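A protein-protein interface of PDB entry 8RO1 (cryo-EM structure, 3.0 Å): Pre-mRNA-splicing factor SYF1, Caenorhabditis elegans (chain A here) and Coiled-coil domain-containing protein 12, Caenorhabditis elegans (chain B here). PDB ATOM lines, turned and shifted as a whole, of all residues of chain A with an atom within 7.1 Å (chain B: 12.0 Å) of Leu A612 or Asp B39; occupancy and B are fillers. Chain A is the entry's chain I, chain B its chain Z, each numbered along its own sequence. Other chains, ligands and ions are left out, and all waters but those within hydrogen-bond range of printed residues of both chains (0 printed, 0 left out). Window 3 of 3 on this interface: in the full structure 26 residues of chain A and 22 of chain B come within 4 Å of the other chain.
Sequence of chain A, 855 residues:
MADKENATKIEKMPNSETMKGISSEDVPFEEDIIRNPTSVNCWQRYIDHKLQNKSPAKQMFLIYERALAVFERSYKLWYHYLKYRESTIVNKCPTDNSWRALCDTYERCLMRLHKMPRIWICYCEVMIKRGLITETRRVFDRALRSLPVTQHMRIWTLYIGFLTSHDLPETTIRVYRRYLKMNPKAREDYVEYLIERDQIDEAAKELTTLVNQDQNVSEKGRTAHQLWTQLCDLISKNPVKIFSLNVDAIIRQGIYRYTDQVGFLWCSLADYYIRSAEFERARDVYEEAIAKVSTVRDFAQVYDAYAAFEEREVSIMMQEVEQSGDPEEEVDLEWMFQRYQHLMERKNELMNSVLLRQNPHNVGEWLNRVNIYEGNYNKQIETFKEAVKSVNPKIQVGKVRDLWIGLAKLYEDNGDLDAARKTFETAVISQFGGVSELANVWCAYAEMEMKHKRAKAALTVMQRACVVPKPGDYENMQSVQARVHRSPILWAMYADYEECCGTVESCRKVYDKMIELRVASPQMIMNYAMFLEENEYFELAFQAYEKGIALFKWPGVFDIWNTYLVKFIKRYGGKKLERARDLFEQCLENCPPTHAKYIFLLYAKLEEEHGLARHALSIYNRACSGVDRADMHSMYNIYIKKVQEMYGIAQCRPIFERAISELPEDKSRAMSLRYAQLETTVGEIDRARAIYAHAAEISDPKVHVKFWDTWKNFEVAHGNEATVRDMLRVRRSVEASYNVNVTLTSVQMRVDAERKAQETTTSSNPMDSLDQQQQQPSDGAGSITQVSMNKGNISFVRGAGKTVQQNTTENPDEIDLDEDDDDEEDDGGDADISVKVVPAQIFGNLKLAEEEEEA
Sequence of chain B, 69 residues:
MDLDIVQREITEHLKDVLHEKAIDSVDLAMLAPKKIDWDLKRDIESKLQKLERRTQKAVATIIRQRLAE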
ATOM      1  N   LEU A 577       2.745  -5.917  -3.506  1.00  0.00           N
ATOM      2  CA  LEU A 577       3.709  -6.156  -4.588  1.00  0.00           C
ATOM      3  C   LEU A 577       4.303  -4.887  -5.194  1.00  0.00           C
ATOM      4  O   LEU A 577       5.489  -4.880  -5.533  1.00  0.00           O
ATOM      5  CB  LEU A 577       3.046  -6.958  -5.706  1.00  0.00           C
ATOM      6  CG  LEU A 577       3.804  -7.097  -7.041  1.00  0.00           C
ATOM      7  CD1 LEU A 577       3.695  -8.507  -7.539  1.00  0.00           C
ATOM      8  CD2 LEU A 577       3.289  -6.134  -8.100  1.00  0.00           C
ATOM      9  N   ARG A 581       8.507  -4.732  -5.147  1.00  0.00           N
ATOM     10  CA  ARG A 581       9.475  -4.496  -6.213  1.00  0.00           C
ATOM     11  C   ARG A 581      10.470  -3.405  -5.861  1.00  0.00           C
ATOM     12  O   ARG A 581      11.637  -3.482  -6.248  1.00  0.00           O
ATOM     13  CB  ARG A 581       8.751  -4.182  -7.514  1.00  0.00           C
ATOM     14  CG  ARG A 581       7.879  -5.331  -7.945  1.00  0.00           C
ATOM     15  CD  ARG A 581       7.423  -5.238  -9.372  1.00  0.00           C
ATOM     16  NE  ARG A 581       6.643  -4.031  -9.593  1.00  0.00           N
ATOM     17  CZ  ARG A 581       5.892  -3.789 -10.657  1.00  0.00           C
ATOM     18  NH1 ARG A 581       5.272  -2.620 -10.752  1.00  0.00           N
ATOM     19  NH2 ARG A 581       5.713  -4.690 -11.610  1.00  0.00           N
ATOM     20  N   LEU A 606       8.592 -13.796  -7.113  1.00  0.00           N
ATOM     21  CA  LEU A 606       7.524 -12.840  -6.847  1.00  0.00           C
ATOM     22  C   LEU A 606       6.871 -12.365  -8.137  1.00  0.00           C
ATOM     23  O   LEU A 606       5.649 -12.426  -8.290  1.00  0.00           O
ATOM     24  CB  LEU A 606       8.071 -11.653  -6.050  1.00  0.00           C
ATOM     25  CG  LEU A 606       7.240 -10.369  -5.902  1.00  0.00           C
ATOM     26  CD1 LEU A 606       6.198 -10.591  -4.837  1.00  0.00           C
ATOM     27  CD2 LEU A 606       8.102  -9.207  -5.525  1.00  0.00           C
ATOM     28  N   GLU A 607       7.684 -11.919  -9.089  1.00  0.00           N
ATOM     29  CA  GLU A 607       7.165 -11.366 -10.335  1.00  0.00           C
ATOM     30  C   GLU A 607       6.544 -12.415 -11.241  1.00  0.00           C
ATOM     31  O   GLU A 607       5.635 -12.092 -12.009  1.00  0.00           O
ATOM     32  CB  GLU A 607       8.267 -10.605 -11.054  1.00  0.00           C
ATOM     33  CG  GLU A 607       8.520  -9.248 -10.417  1.00  0.00           C
ATOM     34  CD  GLU A 607       8.059  -8.077 -11.261  1.00  0.00           C
ATOM     35  OE1 GLU A 607       6.840  -7.817 -11.305  1.00  0.00           O
ATOM     36  OE2 GLU A 607       8.922  -7.381 -11.829  1.00  0.00           O
ATOM     37  N   GLU A 608       7.018 -13.655 -11.198  1.00  0.00           N
ATOM     38  CA  GLU A 608       6.312 -14.718 -11.907  1.00  0.00           C
ATOM     39  C   GLU A 608       4.911 -14.923 -11.348  1.00  0.00           C
ATOM     40  O   GLU A 608       3.918 -14.799 -12.072  1.00  0.00           O
ATOM     41  CB  GLU A 608       7.108 -16.022 -11.839  1.00  0.00           C
ATOM     42  CG  GLU A 608       8.262 -16.125 -12.818  1.00  0.00           C
ATOM     43  CD  GLU A 608       8.808 -17.532 -12.911  1.00  0.00           C
ATOM     44  OE1 GLU A 608       9.639 -17.905 -12.056  1.00  0.00           O
ATOM     45  OE2 GLU A 608       8.409 -18.267 -13.835  1.00  0.00           O
ATOM     46  N   GLU A 609       4.803 -15.250 -10.063  1.00  0.00           N
ATOM     47  CA  GLU A 609       3.527 -15.733  -9.546  1.00  0.00           C
ATOM     48  C   GLU A 609       2.497 -14.610  -9.401  1.00  0.00           C
ATOM     49  O   GLU A 609       1.372 -14.729  -9.898  1.00  0.00           O
ATOM     50  CB  GLU A 609       3.760 -16.493  -8.225  1.00  0.00           C
ATOM     51  CG  GLU A 609       4.031 -15.676  -6.957  1.00  0.00           C
ATOM     52  CD  GLU A 609       4.290 -16.539  -5.739  1.00  0.00           C
ATOM     53  OE1 GLU A 609       3.510 -17.484  -5.503  1.00  0.00           O
ATOM     54  OE2 GLU A 609       5.259 -16.256  -5.003  1.00  0.00           O
ATOM     55  N   HIS A 610       2.859 -13.505  -8.738  1.00  0.00           N
ATOM     56  CA  HIS A 610       1.992 -12.331  -8.671  1.00  0.00           C
ATOM     57  C   HIS A 610       2.106 -11.421  -9.886  1.00  0.00           C
ATOM     58  O   HIS A 610       1.091 -10.952 -10.408  1.00  0.00           O
ATOM     59  CB  HIS A 610       2.309 -11.549  -7.404  1.00  0.00           C
ATOM     60  CG  HIS A 610       2.031 -12.314  -6.152  1.00  0.00           C
ATOM     61  ND1 HIS A 610       3.011 -12.606  -5.230  1.00  0.00           N
ATOM     62  CD2 HIS A 610       0.892 -12.872  -5.681  1.00  0.00           C
ATOM     63  CE1 HIS A 610       2.485 -13.296  -4.235  1.00  0.00           C
ATOM     64  NE2 HIS A 610       1.199 -13.469  -4.482  1.00  0.00           N
ATOM     65  N   GLY A 611       3.314 -11.161 -10.351  1.00  0.00           N
ATOM     66  CA  GLY A 611       3.551 -10.099 -11.304  1.00  0.00           C
ATOM     67  C   GLY A 611       3.231 -10.466 -12.738  1.00  0.00           C
ATOM     68  O   GLY A 611       2.538 -11.444 -13.030  1.00  0.00           O
ATOM     69  N   LEU A 612       3.747  -9.642 -13.642  1.00  0.00           N
ATOM     70  CA  LEU A 612       3.622  -9.825 -15.080  1.00  0.00           C
ATOM     71  C   LEU A 612       4.828 -10.578 -15.639  1.00  0.00           C
ATOM     72  O   LEU A 612       5.951 -10.463 -15.143  1.00  0.00           O
ATOM     73  CB  LEU A 612       3.463  -8.476 -15.772  1.00  0.00           C
ATOM     74  CG  LEU A 612       2.980  -8.463 -17.217  1.00  0.00           C
ATOM     75  CD1 LEU A 612       1.502  -8.799 -17.267  1.00  0.00           C
ATOM     76  CD2 LEU A 612       3.233  -7.113 -17.845  1.00  0.00           C
ATOM     77  N   ALA A 613       4.572 -11.347 -16.698  1.00  0.00           N
ATOM     78  CA  ALA A 613       5.516 -12.351 -17.184  1.00  0.00           C
ATOM     79  C   ALA A 613       6.772 -11.743 -17.806  1.00  0.00           C
ATOM     80  O   ALA A 613       7.885 -12.205 -17.534  1.00  0.00           O
ATOM     81  CB  ALA A 613       4.815 -13.259 -18.191  1.00  0.00           C
ATOM     82  N   ARG A 614       6.619 -10.729 -18.661  1.00  0.00           N
ATOM     83  CA  ARG A 614       7.787 -10.064 -19.248  1.00  0.00           C
ATOM     84  C   ARG A 614       8.726  -9.487 -18.192  1.00  0.00           C
ATOM     85  O   ARG A 614       9.948  -9.527 -18.363  1.00  0.00           O
ATOM     86  CB  ARG A 614       7.351  -8.963 -20.220  1.00  0.00           C
ATOM     87  CG  ARG A 614       7.262  -9.383 -21.704  1.00  0.00           C
ATOM     88  CD  ARG A 614       8.628  -9.680 -22.360  1.00  0.00           C
ATOM     89  NE  ARG A 614       8.501 -10.049 -23.771  1.00  0.00           N
ATOM     90  CZ  ARG A 614       9.507 -10.377 -24.578  1.00  0.00           C
ATOM     91  NH1 ARG A 614       9.248 -10.692 -25.844  1.00  0.00           N
ATOM     92  NH2 ARG A 614      10.764 -10.393 -24.160  1.00  0.00           N
ATOM     93  N   HIS A 615       8.191  -8.940 -17.100  1.00  0.00           N
ATOM     94  CA  HIS A 615       9.068  -8.429 -16.047  1.00  0.00           C
ATOM     95  C   HIS A 615       9.863  -9.540 -15.369  1.00  0.00           C
ATOM     96  O   HIS A 615      11.033  -9.345 -15.028  1.00  0.00           O
ATOM     97  CB  HIS A 615       8.283  -7.664 -14.986  1.00  0.00           C
ATOM     98  CG  HIS A 615       7.557  -6.465 -15.501  1.00  0.00           C
ATOM     99  ND1 HIS A 615       8.190  -5.456 -16.191  1.00  0.00           N
ATOM    100  CD2 HIS A 615       6.270  -6.076 -15.362  1.00  0.00           C
ATOM    101  CE1 HIS A 615       7.311  -4.519 -16.498  1.00  0.00           C
ATOM    102  NE2 HIS A 615       6.137  -4.874 -16.011  1.00  0.00           N
ATOM    103  N   ALA A 616       9.251 -10.702 -15.151  1.00  0.00           N
ATOM    104  CA  ALA A 616       9.987 -11.834 -14.595  1.00  0.00           C
ATOM    105  C   ALA A 616      11.137 -12.282 -15.492  1.00  0.00           C
ATOM    106  O   ALA A 616      12.246 -12.535 -15.012  1.00  0.00           O
ATOM    107  CB  ALA A 616       9.030 -12.999 -14.353  1.00  0.00           C
ATOM    108  N   LEU A 617      10.897 -12.384 -16.796  1.00  0.00           N
ATOM    109  CA  LEU A 617      11.972 -12.728 -17.725  1.00  0.00           C
ATOM    110  C   LEU A 617      13.070 -11.674 -17.765  1.00  0.00           C
ATOM    111  O   LEU A 617      14.253 -12.011 -17.880  1.00  0.00           O
ATOM    112  CB  LEU A 617      11.394 -12.928 -19.122  1.00  0.00           C
ATOM    113  CG  LEU A 617      10.430 -14.098 -19.311  1.00  0.00           C
ATOM    114  CD1 LEU A 617       9.954 -14.117 -20.744  1.00  0.00           C
ATOM    115  CD2 LEU A 617      11.066 -15.426 -18.945  1.00  0.00           C
ATOM    116  N   ILE A 619      14.150  -9.945 -15.339  1.00  0.00           N
ATOM    117  CA  ILE A 619      14.998 -10.136 -14.169  1.00  0.00           C
ATOM    118  C   ILE A 619      16.072 -11.185 -14.437  1.00  0.00           C
ATOM    119  O   ILE A 619      17.213 -11.050 -13.982  1.00  0.00           O
ATOM    120  CB  ILE A 619      14.105 -10.507 -12.971  1.00  0.00           C
ATOM    121  CG1 ILE A 619      13.318  -9.272 -12.519  1.00  0.00           C
ATOM    122  CG2 ILE A 619      14.926 -11.054 -11.804  1.00  0.00           C
ATOM    123  CD1 ILE A 619      12.071  -9.578 -11.720  1.00  0.00           C
ATOM    124  N   MET A 646       7.283 -20.910 -21.725  1.00  0.00           N
ATOM    125  CA  MET A 646       6.150 -20.055 -22.094  1.00  0.00           C
ATOM    126  C   MET A 646       6.114 -19.622 -23.553  1.00  0.00           C
ATOM    127  O   MET A 646       5.044 -19.693 -24.160  1.00  0.00           O
ATOM    128  CB  MET A 646       6.099 -18.821 -21.172  1.00  0.00           C
ATOM    129  CG  MET A 646       7.187 -17.772 -21.322  1.00  0.00           C
ATOM    130  SD  MET A 646       6.882 -16.353 -20.256  1.00  0.00           S
ATOM    131  CE  MET A 646       7.346 -17.015 -18.661  1.00  0.00           C
ATOM    132  N   TYR A 647       7.227 -19.195 -24.156  1.00  0.00           N
ATOM    133  CA  TYR A 647       7.232 -18.715 -25.537  1.00  0.00           C
ATOM    134  C   TYR A 647       7.811 -19.714 -26.531  1.00  0.00           C
ATOM    135  O   TYR A 647       7.897 -19.398 -27.720  1.00  0.00           O
ATOM    136  CB  TYR A 647       7.998 -17.390 -25.650  1.00  0.00           C
ATOM    137  CG  TYR A 647       7.498 -16.255 -24.775  1.00  0.00           C
ATOM    138  CD1 TYR A 647       6.150 -16.094 -24.496  1.00  0.00           C
ATOM    139  CD2 TYR A 647       8.382 -15.323 -24.255  1.00  0.00           C
ATOM    140  CE1 TYR A 647       5.707 -15.055 -23.710  1.00  0.00           C
ATOM    141  CE2 TYR A 647       7.943 -14.281 -23.468  1.00  0.00           C
ATOM    142  CZ  TYR A 647       6.607 -14.156 -23.193  1.00  0.00           C
ATOM    143  OH  TYR A 647       6.165 -13.124 -22.398  1.00  0.00           O
ATOM    144  N   HIS B  13      12.865 -23.103  -8.053  1.00  0.00           N
ATOM    145  CA  HIS B  13      13.851 -22.653  -9.036  1.00  0.00           C
ATOM    146  C   HIS B  13      15.160 -23.422  -8.925  1.00  0.00           C
ATOM    147  O   HIS B  13      15.727 -23.854  -9.935  1.00  0.00           O
ATOM    148  CB  HIS B  13      14.069 -21.147  -8.914  1.00  0.00           C
ATOM    149  CG  HIS B  13      12.814 -20.354  -9.093  1.00  0.00           C
ATOM    150  ND1 HIS B  13      11.845 -20.256  -8.119  1.00  0.00           N
ATOM    151  CD2 HIS B  13      12.362 -19.634 -10.147  1.00  0.00           C
ATOM    152  CE1 HIS B  13      10.852 -19.509  -8.565  1.00  0.00           C
ATOM    153  NE2 HIS B  13      11.143 -19.115  -9.791  1.00  0.00           N
ATOM    154  N   PRO B  33       3.723 -23.020 -26.379  1.00  0.00           N
ATOM    155  CA  PRO B  33       2.859 -23.551 -25.319  1.00  0.00           C
ATOM    156  C   PRO B  33       1.948 -22.516 -24.685  1.00  0.00           C
ATOM    157  O   PRO B  33       0.865 -22.883 -24.215  1.00  0.00           O
ATOM    158  CB  PRO B  33       3.859 -24.110 -24.302  1.00  0.00           C
ATOM    159  CG  PRO B  33       5.088 -23.327 -24.516  1.00  0.00           C
ATOM    160  CD  PRO B  33       5.136 -22.997 -25.973  1.00  0.00           C
ATOM    161  N   LYS B  34       2.353 -21.246 -24.642  1.00  0.00           N
ATOM    162  CA  LYS B  34       1.471 -20.143 -24.281  1.00  0.00           C
ATOM    163  C   LYS B  34       1.500 -19.045 -25.332  1.00  0.00           C
ATOM    164  O   LYS B  34       2.547 -18.756 -25.915  1.00  0.00           O
ATOM    165  CB  LYS B  34       1.874 -19.572 -22.925  1.00  0.00           C
ATOM    166  CG  LYS B  34       1.722 -20.557 -21.785  1.00  0.00           C
ATOM    167  CD  LYS B  34       2.011 -19.902 -20.455  1.00  0.00           C
ATOM    168  CE  LYS B  34       1.820 -20.871 -19.308  1.00  0.00           C
ATOM    169  NZ  LYS B  34       2.150 -20.232 -18.008  1.00  0.00           N
ATOM    170  N   LYS B  35       0.337 -18.449 -25.578  1.00  0.00           N
ATOM    171  CA  LYS B  35       0.238 -17.320 -26.490  1.00  0.00           C
ATOM    172  C   LYS B  35       0.954 -16.106 -25.913  1.00  0.00           C
ATOM    173  O   LYS B  35       1.036 -15.930 -24.697  1.00  0.00           O
ATOM    174  CB  LYS B  35      -1.222 -16.946 -26.731  1.00  0.00           C
ATOM    175  CG  LYS B  35      -2.109 -18.032 -27.301  1.00  0.00           C
ATOM    176  CD  LYS B  35      -1.727 -18.405 -28.718  1.00  0.00           C
ATOM    177  CE  LYS B  35      -2.605 -19.526 -29.240  1.00  0.00           C
ATOM    178  NZ  LYS B  35      -4.027 -19.103 -29.388  1.00  0.00           N
ATOM    179  N   ILE B  36       1.480 -15.254 -26.795  1.00  0.00           N
ATOM    180  CA  ILE B  36       2.286 -14.086 -26.413  1.00  0.00           C
ATOM    181  C   ILE B  36       1.507 -13.023 -25.625  1.00  0.00           C
ATOM    182  O   ILE B  36       2.103 -12.053 -25.165  1.00  0.00           O
ATOM    183  CB  ILE B  36       3.008 -13.469 -27.630  1.00  0.00           C
ATOM    184  CG1 ILE B  36       2.044 -12.772 -28.612  1.00  0.00           C
ATOM    185  CG2 ILE B  36       3.876 -14.530 -28.324  1.00  0.00           C
ATOM    186  CD1 ILE B  36       2.777 -11.935 -29.662  1.00  0.00           C
ATOM    187  N   ASP B  37       0.194 -13.193 -25.456  1.00  0.00           N
ATOM    188  CA  ASP B  37      -0.670 -12.281 -24.717  1.00  0.00           C
ATOM    189  C   ASP B  37      -1.244 -12.915 -23.456  1.00  0.00           C
ATOM    190  O   ASP B  37      -2.116 -12.313 -22.821  1.00  0.00           O
ATOM    191  CB  ASP B  37      -1.798 -11.782 -25.621  1.00  0.00           C
ATOM    192  CG  ASP B  37      -2.701 -12.897 -26.106  1.00  0.00           C
ATOM    193  OD1 ASP B  37      -2.331 -14.078 -25.957  1.00  0.00           O
ATOM    194  OD2 ASP B  37      -3.785 -12.590 -26.639  1.00  0.00           O
ATOM    195  N   TRP B  38      -0.801 -14.131 -23.110  1.00  0.00           N
ATOM    196  CA  TRP B  38      -1.457 -14.957 -22.101  1.00  0.00           C
ATOM    197  C   TRP B  38      -1.576 -14.262 -20.752  1.00  0.00           C
ATOM    198  O   TRP B  38      -2.553 -14.489 -20.030  1.00  0.00           O
ATOM    199  CB  TRP B  38      -0.705 -16.284 -21.955  1.00  0.00           C
ATOM    200  CG  TRP B  38       0.573 -16.191 -21.180  1.00  0.00           C
ATOM    201  CD1 TRP B  38       1.812 -15.945 -21.679  1.00  0.00           C
ATOM    202  CD2 TRP B  38       0.732 -16.337 -19.766  1.00  0.00           C
ATOM    203  NE1 TRP B  38       2.733 -15.920 -20.667  1.00  0.00           N
ATOM    204  CE2 TRP B  38       2.097 -16.175 -19.482  1.00  0.00           C
ATOM    205  CE3 TRP B  38      -0.147 -16.602 -18.717  1.00  0.00           C
ATOM    206  CZ2 TRP B  38       2.602 -16.261 -18.192  1.00  0.00           C
ATOM    207  CZ3 TRP B  38       0.357 -16.689 -17.439  1.00  0.00           C
ATOM    208  CH2 TRP B  38       1.718 -16.519 -17.186  1.00  0.00           C
ATOM    209  N   ASP B  39      -0.611 -13.417 -20.392  1.00  0.00           N
ATOM    210  CA  ASP B  39      -0.656 -12.756 -19.096  1.00  0.00           C
ATOM    211  C   ASP B  39      -1.487 -11.487 -19.108  1.00  0.00           C
ATOM    212  O   ASP B  39      -1.999 -11.097 -18.054  1.00  0.00           O
ATOM    213  CB  ASP B  39       0.760 -12.415 -18.619  1.00  0.00           C
ATOM    214  CG  ASP B  39       1.505 -11.526 -19.592  1.00  0.00           C
ATOM    215  OD1 ASP B  39       1.055 -11.416 -20.749  1.00  0.00           O
ATOM    216  OD2 ASP B  39       2.542 -10.949 -19.207  1.00  0.00           O
ATOM    217  N   LEU B  40      -1.649 -10.837 -20.261  1.00  0.00           N
ATOM    218  CA  LEU B  40      -2.619  -9.751 -20.332  1.00  0.00           C
ATOM    219  C   LEU B  40      -4.025 -10.309 -20.201  1.00  0.00           C
ATOM    220  O   LEU B  40      -4.880  -9.723 -19.530  1.00  0.00           O
ATOM    221  CB  LEU B  40      -2.460  -8.981 -21.640  1.00  0.00           C
ATOM    222  CG  LEU B  40      -1.119  -8.292 -21.893  1.00  0.00           C
ATOM    223  CD1 LEU B  40      -1.138  -7.621 -23.247  1.00  0.00           C
ATOM    224  CD2 LEU B  40      -0.798  -7.269 -20.814  1.00  0.00           C
ATOM    225  N   LYS B  41      -4.272 -11.445 -20.852  1.00  0.00           N
ATOM    226  CA  LYS B  41      -5.550 -12.136 -20.748  1.00  0.00           C
ATOM    227  C   LYS B  41      -5.833 -12.551 -19.312  1.00  0.00           C
ATOM    228  O   LYS B  41      -6.975 -12.474 -18.847  1.00  0.00           O
ATOM    229  CB  LYS B  41      -5.545 -13.339 -21.692  1.00  0.00           C
ATOM    230  CG  LYS B  41      -6.905 -14.024 -21.917  1.00  0.00           C
ATOM    231  CD  LYS B  41      -7.316 -15.086 -20.878  1.00  0.00           C
ATOM    232  CE  LYS B  41      -6.328 -16.246 -20.774  1.00  0.00           C
ATOM    233  NZ  LYS B  41      -6.936 -17.451 -20.152  1.00  0.00           N
ATOM    234  N   ARG B  42      -4.805 -13.024 -18.606  1.00  0.00           N
ATOM    235  CA  ARG B  42      -4.947 -13.423 -17.208  1.00  0.00           C
ATOM    236  C   ARG B  42      -5.443 -12.272 -16.339  1.00  0.00           C
ATOM    237  O   ARG B  42      -6.364 -12.443 -15.535  1.00  0.00           O
ATOM    238  CB  ARG B  42      -3.598 -13.947 -16.713  1.00  0.00           C
ATOM    239  CG  ARG B  42      -3.531 -14.469 -15.269  1.00  0.00           C
ATOM    240  CD  ARG B  42      -2.096 -14.436 -14.761  1.00  0.00           C
ATOM    241  NE  ARG B  42      -1.615 -13.068 -14.595  1.00  0.00           N
ATOM    242  CZ  ARG B  42      -0.362 -12.718 -14.339  1.00  0.00           C
ATOM    243  NH1 ARG B  42      -0.064 -11.427 -14.226  1.00  0.00           N
ATOM    244  NH2 ARG B  42       0.602 -13.616 -14.196  1.00  0.00           N
ATOM    245  N   ASP B  43      -4.846 -11.089 -16.481  1.00  0.00           N
ATOM    246  CA  ASP B  43      -5.243  -9.956 -15.652  1.00  0.00           C
ATOM    247  C   ASP B  43      -6.640  -9.439 -15.971  1.00  0.00           C
ATOM    248  O   ASP B  43      -7.243  -8.769 -15.127  1.00  0.00           O
ATOM    249  CB  ASP B  43      -4.240  -8.814 -15.813  1.00  0.00           C
ATOM    250  CG  ASP B  43      -2.912  -9.106 -15.145  1.00  0.00           C
ATOM    251  OD1 ASP B  43      -2.721 -10.239 -14.662  1.00  0.00           O
ATOM    252  OD2 ASP B  43      -2.058  -8.195 -15.099  1.00  0.00           O
ATOM    253  N   ILE B  44      -7.165  -9.733 -17.159  1.00  0.00           N
ATOM    254  CA  ILE B  44      -8.525  -9.334 -17.511  1.00  0.00           C
ATOM    255  C   ILE B  44      -9.569 -10.311 -16.965  1.00  0.00           C
ATOM    256  O   ILE B  44     -10.718  -9.917 -16.738  1.00  0.00           O
ATOM    257  CB  ILE B  44      -8.601  -9.152 -19.042  1.00  0.00           C
ATOM    258  CG1 ILE B  44      -7.998  -7.787 -19.397  1.00  0.00           C
ATOM    259  CG2 ILE B  44     -10.039  -9.292 -19.582  1.00  0.00           C
ATOM    260  CD1 ILE B  44      -7.751  -7.536 -20.873  1.00  0.00           C
ATOM    261  N   GLU B  45      -9.206 -11.583 -16.761  1.00  0.00           N
ATOM    262  CA  GLU B  45     -10.197 -12.634 -16.523  1.00  0.00           C
ATOM    263  C   GLU B  45     -11.045 -12.406 -15.277  1.00  0.00           C
ATOM    264  O   GLU B  45     -12.220 -12.790 -15.261  1.00  0.00           O
ATOM    265  CB  GLU B  45      -9.521 -13.997 -16.407  1.00  0.00           C
ATOM    266  CG  GLU B  45      -9.499 -14.771 -17.701  1.00  0.00           C
ATOM    267  CD  GLU B  45      -8.833 -16.123 -17.555  1.00  0.00           C
ATOM    268  OE1 GLU B  45      -8.147 -16.343 -16.534  1.00  0.00           O
ATOM    269  OE2 GLU B  45      -8.994 -16.968 -18.461  1.00  0.00           O
ATOM    270  N   SER B  46     -10.488 -11.805 -14.227  1.00  0.00           N
ATOM    271  CA  SER B  46     -11.322 -11.494 -13.069  1.00  0.00           C
ATOM    272  C   SER B  46     -12.395 -10.472 -13.419  1.00  0.00           C
ATOM    273  O   SER B  46     -13.552 -10.619 -13.013  1.00  0.00           O
ATOM    274  CB  SER B  46     -10.454 -10.978 -11.923  1.00  0.00           C
ATOM    275  OG  SER B  46     -10.190  -9.593 -12.065  1.00  0.00           O
ATOM    276  N   LYS B  47     -12.039  -9.442 -14.185  1.00  0.00           N
ATOM    277  CA  LYS B  47     -13.018  -8.439 -14.579  1.00  0.00           C
ATOM    278  C   LYS B  47     -13.934  -8.942 -15.685  1.00  0.00           C
ATOM    279  O   LYS B  47     -15.107  -8.559 -15.739  1.00  0.00           O
ATOM    280  CB  LYS B  47     -12.307  -7.164 -15.032  1.00  0.00           C
ATOM    281  CG  LYS B  47     -11.638  -6.397 -13.898  1.00  0.00           C
ATOM    282  CD  LYS B  47     -11.016  -5.087 -14.374  1.00  0.00           C
ATOM    283  CE  LYS B  47      -9.800  -5.300 -15.259  1.00  0.00           C
ATOM    284  NZ  LYS B  47      -9.074  -4.022 -15.501  1.00  0.00           N
ATOM    285  N   LEU B  48     -13.416  -9.795 -16.565  1.00  0.00           N
ATOM    286  CA  LEU B  48     -14.185 -10.293 -17.699  1.00  0.00           C
ATOM    287  C   LEU B  48     -15.388 -11.128 -17.271  1.00  0.00           C
ATOM    288  O   LEU B  48     -16.419 -11.119 -17.952  1.00  0.00           O
ATOM    289  CB  LEU B  48     -13.270 -11.099 -18.614  1.00  0.00           C
ATOM    290  CG  LEU B  48     -13.828 -11.583 -19.950  1.00  0.00           C
ATOM    291  CD1 LEU B  48     -14.179 -10.407 -20.843  1.00  0.00           C
ATOM    292  CD2 LEU B  48     -12.822 -12.475 -20.632  1.00  0.00           C
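The side-chain carboxylate of Glu A608 lies within hydrogen-bond range of a ring nitrogen (NE2) of His B13, at 3.0 Å. The backbone NH (N) of Lys B34 is in hydrogen-bond range of the backbone carbonyl oxygen (O) of Met A646 (3.1 Å). OD2 of Asp B39 sits at hydrogen-bond distance from N of Ala A613. The guanidinium group (NH1) of Arg B42 lies within hydrogen-bond range of the backbone carbonyl oxygen (O) of Gly A611 (2.9 Å).
OD1 of Asp B43 lies within salt-bridge range of NH1 of Arg B42 (2.9 Å). The backbone carbonyl oxygen of Leu A606 lies within hydrogen-bond range of the backbone NH of Gly A611 (3.4 Å). The backbone carbonyl oxygen (O) of Glu A607 is in hydrogen-bond range of the backbone NH (N) of Leu A612 (3.5 Å).
Among the printed residues, pairs that only touch across the chains: Leu A612 with Asp B39 (3.1 Å), Met A646 with Pro B33 (3.7 Å) and Ala A613 with Trp B38 (3.7 Å).
Glu A609 touches none of the printed residues of chain B. Gly A611 touches just one residue of chain B: Arg B42. Of the printed residues of chain B, Leu A612 touches Asp B39. Of chain B, only Trp B38 and Asp B39 come within 4 Å of Ala A613. Of the printed residues of chain B, Met A646 touches Pro B33 (3.7 Å) and Lys B34 (3.1 Å). Of the printed residues of chain A, His B13 touches Glu A608. Printed residues of chain A within 4 Å of Pro B33: Met A646. Printed residues of chain A within 4 Å of Trp B38: Ala A613 (3.7 Å). Asp B39 touches just these residues of chain A: Leu A612 and Ala A613. Asp B43 touches none of the printed residues of chain A. The nearest residue of chain B that does not touch Leu A612 is Arg B42 (4.1 Å). The nearest printed residue of chain A that does not touch Arg B42 is His A610 (4.02 Å).
Of the 17 printed residues of chain B, 6 touch a printed residue of chain A. Printed residues of chain B that touch a printed residue of chain A: His B13, Pro B33, Lys B34, Trp B38, Asp B39 and Arg B42. Hydrophobic or aromatic side chains of chain B within 4 Å of the printed part of chain A: His B13, Pro B33 and Trp B38. Printed residues of chain A that touch a printed residue of chain B: Glu A608, Gly A611, Leu A612, Ala A613 and Met A646. Among the printed residues, no Asp or Glu carboxylate lies within 4 Å of a Lys or Arg side-chain nitrogen of the other chain.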
